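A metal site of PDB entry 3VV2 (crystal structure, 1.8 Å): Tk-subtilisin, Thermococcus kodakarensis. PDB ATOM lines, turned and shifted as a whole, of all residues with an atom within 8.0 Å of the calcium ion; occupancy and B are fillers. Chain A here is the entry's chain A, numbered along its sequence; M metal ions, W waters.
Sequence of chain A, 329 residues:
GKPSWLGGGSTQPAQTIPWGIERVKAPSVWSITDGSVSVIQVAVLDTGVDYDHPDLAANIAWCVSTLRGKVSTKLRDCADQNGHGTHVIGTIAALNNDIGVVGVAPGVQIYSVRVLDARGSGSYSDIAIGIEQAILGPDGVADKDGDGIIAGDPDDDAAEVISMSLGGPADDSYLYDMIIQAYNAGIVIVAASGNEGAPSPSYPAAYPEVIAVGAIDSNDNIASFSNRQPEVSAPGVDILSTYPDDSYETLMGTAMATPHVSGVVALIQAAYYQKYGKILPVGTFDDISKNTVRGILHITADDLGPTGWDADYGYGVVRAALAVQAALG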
ATOM      1  N   ASP A 302      17.760  31.469 -21.951  1.00  0.00           N
ATOM      2  CA  ASP A 302      16.743  32.461 -22.310  1.00  0.00           C
ATOM      3  C   ASP A 302      15.528  32.103 -21.478  1.00  0.00           C
ATOM      4  O   ASP A 302      14.839  31.104 -21.751  1.00  0.00           O
ATOM      5  CB  ASP A 302      16.468  32.370 -23.803  1.00  0.00           C
ATOM      6  CG  ASP A 302      15.585  33.555 -24.320  1.00  0.00           C
ATOM      7  OD1 ASP A 302      15.317  34.457 -23.522  1.00  0.00           O
ATOM      8  OD2 ASP A 302      15.181  33.562 -25.522  1.00  0.00           O
ATOM      9  N   ASP A 303      15.330  32.890 -20.408  1.00  0.00           N
ATOM     10  CA  ASP A 303      14.205  32.702 -19.477  1.00  0.00           C
ATOM     11  C   ASP A 303      12.971  33.005 -20.296  1.00  0.00           C
ATOM     12  O   ASP A 303      12.687  34.189 -20.641  1.00  0.00           O
ATOM     13  CB  ASP A 303      14.439  33.576 -18.256  1.00  0.00           C
ATOM     14  CG  ASP A 303      13.323  33.445 -17.205  1.00  0.00           C
ATOM     15  OD1 ASP A 303      12.473  32.504 -17.242  1.00  0.00           O
ATOM     16  OD2 ASP A 303      13.330  34.291 -16.315  1.00  0.00           O
ATOM     17  N   LEU A 304      12.160  31.967 -20.495  1.00  0.00           N
ATOM     18  CA  LEU A 304      10.912  32.114 -21.194  1.00  0.00           C
ATOM     19  C   LEU A 304       9.854  31.892 -20.118  1.00  0.00           C
ATOM     20  O   LEU A 304      10.175  31.548 -18.988  1.00  0.00           O
ATOM     21  CB  LEU A 304      10.709  31.169 -22.376  1.00  0.00           C
ATOM     22  CG  LEU A 304      11.747  31.361 -23.481  1.00  0.00           C
ATOM     23  CD1 LEU A 304      11.412  30.422 -24.581  1.00  0.00           C
ATOM     24  CD2 LEU A 304      11.721  32.832 -23.964  1.00  0.00           C
ATOM     25  N   GLY A 305       8.595  32.131 -20.493  1.00  0.00           N
ATOM     26  CA  GLY A 305       7.462  31.781 -19.604  1.00  0.00           C
ATOM     27  C   GLY A 305       7.460  32.638 -18.373  1.00  0.00           C
ATOM     28  O   GLY A 305       8.024  33.742 -18.414  1.00  0.00           O
ATOM     29  N   PRO A 306       6.802  32.171 -17.270  1.00  0.00           N
ATOM     30  CA  PRO A 306       6.907  32.886 -15.991  1.00  0.00           C
ATOM     31  C   PRO A 306       8.342  33.079 -15.612  1.00  0.00           C
ATOM     32  O   PRO A 306       9.209  32.253 -15.997  1.00  0.00           O
ATOM     33  CB  PRO A 306       6.268  31.913 -14.997  1.00  0.00           C
ATOM     34  CG  PRO A 306       5.182  31.228 -15.839  1.00  0.00           C
ATOM     35  CD  PRO A 306       5.806  31.076 -17.222  1.00  0.00           C
ATOM     36  N   THR A 307       8.605  34.116 -14.812  1.00  0.00           N
ATOM     37  CA  THR A 307       9.959  34.514 -14.440  1.00  0.00           C
ATOM     38  C   THR A 307      10.743  33.422 -13.736  1.00  0.00           C
ATOM     39  O   THR A 307      10.280  32.822 -12.780  1.00  0.00           O
ATOM     40  CB  THR A 307       9.959  35.810 -13.553  1.00  0.00           C
ATOM     41  OG1 THR A 307       9.435  36.894 -14.317  1.00  0.00           O
ATOM     42  CG2 THR A 307      11.353  36.156 -13.088  1.00  0.00           C
ATOM     43  N   GLY A 308      11.964  33.178 -14.235  1.00  0.00           N
ATOM     44  CA  GLY A 308      12.838  32.240 -13.556  1.00  0.00           C
ATOM     45  C   GLY A 308      12.448  30.848 -14.039  1.00  0.00           C
ATOM     46  O   GLY A 308      11.811  30.694 -15.167  1.00  0.00           O
ATOM     47  N   TRP A 309      12.863  29.881 -13.226  1.00  0.00           N
ATOM     48  CA  TRP A 309      12.607  28.444 -13.480  1.00  0.00           C
ATOM     49  C   TRP A 309      11.132  28.238 -13.339  1.00  0.00           C
ATOM     50  O   TRP A 309      10.524  28.740 -12.381  1.00  0.00           O
ATOM     51  CB  TRP A 309      13.313  27.531 -12.467  1.00  0.00           C
ATOM     52  CG  TRP A 309      13.034  26.034 -12.786  1.00  0.00           C
ATOM     53  CD1 TRP A 309      13.835  25.182 -13.526  1.00  0.00           C
ATOM     54  CD2 TRP A 309      11.855  25.258 -12.425  1.00  0.00           C
ATOM     55  NE1 TRP A 309      13.236  23.946 -13.638  1.00  0.00           N
ATOM     56  CE2 TRP A 309      12.038  23.952 -12.960  1.00  0.00           C
ATOM     57  CE3 TRP A 309      10.710  25.525 -11.663  1.00  0.00           C
ATOM     58  CZ2 TRP A 309      11.091  22.936 -12.796  1.00  0.00           C
ATOM     59  CZ3 TRP A 309       9.768  24.510 -11.486  1.00  0.00           C
ATOM     60  CH2 TRP A 309       9.944  23.248 -12.057  1.00  0.00           C
ATOM     61  N   ASP A 310      10.579  27.516 -14.297  1.00  0.00           N
ATOM     62  CA  ASP A 310       9.171  27.224 -14.347  1.00  0.00           C
ATOM     63  C   ASP A 310       8.940  25.812 -14.905  1.00  0.00           C
ATOM     64  O   ASP A 310       9.865  25.150 -15.469  1.00  0.00           O
ATOM     65  CB  ASP A 310       8.426  28.248 -15.192  1.00  0.00           C
ATOM     66  CG  ASP A 310       8.795  28.173 -16.681  1.00  0.00           C
ATOM     67  OD1 ASP A 310       9.639  29.001 -17.109  1.00  0.00           O
ATOM     68  OD2 ASP A 310       8.215  27.339 -17.413  1.00  0.00           O
ATOM     69  N   ALA A 311       7.685  25.361 -14.757  1.00  0.00           N
ATOM     70  CA  ALA A 311       7.359  23.964 -14.978  1.00  0.00           C
ATOM     71  C   ALA A 311       7.350  23.614 -16.449  1.00  0.00           C
ATOM     72  O   ALA A 311       7.348  22.446 -16.774  1.00  0.00           O
ATOM     73  CB  ALA A 311       5.970  23.633 -14.348  1.00  0.00           C
ATOM     74  N   ASP A 312       7.284  24.625 -17.321  1.00  0.00           N
ATOM     75  CA  ASP A 312       7.308  24.384 -18.747  1.00  0.00           C
ATOM     76  C   ASP A 312       8.738  24.376 -19.272  1.00  0.00           C
ATOM     77  O   ASP A 312       9.184  23.385 -19.860  1.00  0.00           O
ATOM     78  CB  ASP A 312       6.470  25.428 -19.500  1.00  0.00           C
ATOM     79  CG  ASP A 312       4.954  25.187 -19.359  1.00  0.00           C
ATOM     80  OD1 ASP A 312       4.572  24.059 -18.920  1.00  0.00           O
ATOM     81  OD2 ASP A 312       4.165  26.131 -19.724  1.00  0.00           O
ATOM     82  N   TYR A 313       9.458  25.458 -19.026  1.00  0.00           N
ATOM     83  CA  TYR A 313      10.743  25.667 -19.739  1.00  0.00           C
ATOM     84  C   TYR A 313      11.946  25.295 -18.886  1.00  0.00           C
ATOM     85  O   TYR A 313      13.106  25.372 -19.358  1.00  0.00           O
ATOM     86  CB  TYR A 313      10.871  27.158 -20.187  1.00  0.00           C
ATOM     87  CG  TYR A 313       9.835  27.630 -21.197  1.00  0.00           C
ATOM     88  CD1 TYR A 313       8.737  28.423 -20.802  1.00  0.00           C
ATOM     89  CD2 TYR A 313       9.945  27.302 -22.504  1.00  0.00           C
ATOM     90  CE1 TYR A 313       7.798  28.852 -21.734  1.00  0.00           C
ATOM     91  CE2 TYR A 313       9.029  27.716 -23.442  1.00  0.00           C
ATOM     92  CZ  TYR A 313       7.958  28.501 -23.055  1.00  0.00           C
ATOM     93  OH  TYR A 313       7.091  28.906 -24.052  1.00  0.00           O
ATOM     94  N   GLY A 314      11.727  24.868 -17.655  1.00  0.00           N
ATOM     95  CA  GLY A 314      12.831  24.822 -16.698  1.00  0.00           C
ATOM     96  C   GLY A 314      13.496  26.188 -16.574  1.00  0.00           C
ATOM     97  O   GLY A 314      12.787  27.169 -16.499  1.00  0.00           O
ATOM     98  N   TYR A 315      14.836  26.263 -16.553  1.00  0.00           N
ATOM     99  CA  TYR A 315      15.487  27.578 -16.481  1.00  0.00           C
ATOM    100  C   TYR A 315      15.372  28.336 -17.815  1.00  0.00           C
ATOM    101  O   TYR A 315      15.643  29.521 -17.885  1.00  0.00           O
ATOM    102  CB  TYR A 315      16.979  27.454 -16.120  1.00  0.00           C
ATOM    103  CG  TYR A 315      17.239  27.195 -14.674  1.00  0.00           C
ATOM    104  CD1 TYR A 315      17.472  25.886 -14.228  1.00  0.00           C
ATOM    105  CD2 TYR A 315      17.228  28.255 -13.744  1.00  0.00           C
ATOM    106  CE1 TYR A 315      17.707  25.602 -12.914  1.00  0.00           C
ATOM    107  CE2 TYR A 315      17.458  28.009 -12.378  1.00  0.00           C
ATOM    108  CZ  TYR A 315      17.675  26.665 -11.970  1.00  0.00           C
ATOM    109  OH  TYR A 315      17.942  26.312 -10.654  1.00  0.00           O
ATOM    110  N   GLY A 316      15.052  27.648 -18.878  1.00  0.00           N
ATOM    111  CA  GLY A 316      14.985  28.340 -20.156  1.00  0.00           C
ATOM    112  C   GLY A 316      15.655  27.569 -21.275  1.00  0.00           C
ATOM    113  O   GLY A 316      16.025  26.416 -21.090  1.00  0.00           O
ATOM    114  N   VAL A 317      15.730  28.226 -22.423  1.00  0.00           N
ATOM    115  CA  VAL A 317      16.333  27.683 -23.628  1.00  0.00           C
ATOM    116  C   VAL A 317      17.830  27.906 -23.527  1.00  0.00           C
ATOM    117  O   VAL A 317      18.303  29.010 -23.549  1.00  0.00           O
ATOM    118  CB  VAL A 317      15.749  28.260 -24.936  1.00  0.00           C
ATOM    119  CG1 VAL A 317      16.452  27.587 -26.223  1.00  0.00           C
ATOM    120  CG2 VAL A 317      14.144  28.138 -24.944  1.00  0.00           C
HETATM  121 CA    CA M   1      10.856  31.019 -17.033  1.00  0.00          CA
HETATM  122  O   HOH W   1      12.578  29.644 -17.842  1.00  0.00           O
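OD2 of Asp 310 sits at hydrogen-bond distance from N of Asp 312, 2.9 Å away.
OD2 of Asp 310 sits at hydrogen-bond distance from N of Tyr 313 (2.8 Å).
Merely in contact with the calcium ion: Gly 305.
Six residues have an atom within 4 Å of the calcium ion: Asp 303, Leu 304, Gly 305, Pro 306, Gly 308 and Asp 310.
The nearest printed residue that does not touch the calcium ion is Thr 307 (4.1 Å).
The calcium ion is bound by O of Gly 308, 2.1 Å away.
The backbone carbonyl oxygen (O) of Leu 304 is bound to the calcium ion, 2.1 Å away.
The calcium ion is bound by OD1 of Asp 303 (2.2 Å).
The backbone carbonyl oxygen (O) of Pro 306 is bound to the calcium ion (2.3 Å).
Water W1 is bound to the calcium ion.
OD1 of Asp 310 is bound to the calcium ion.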
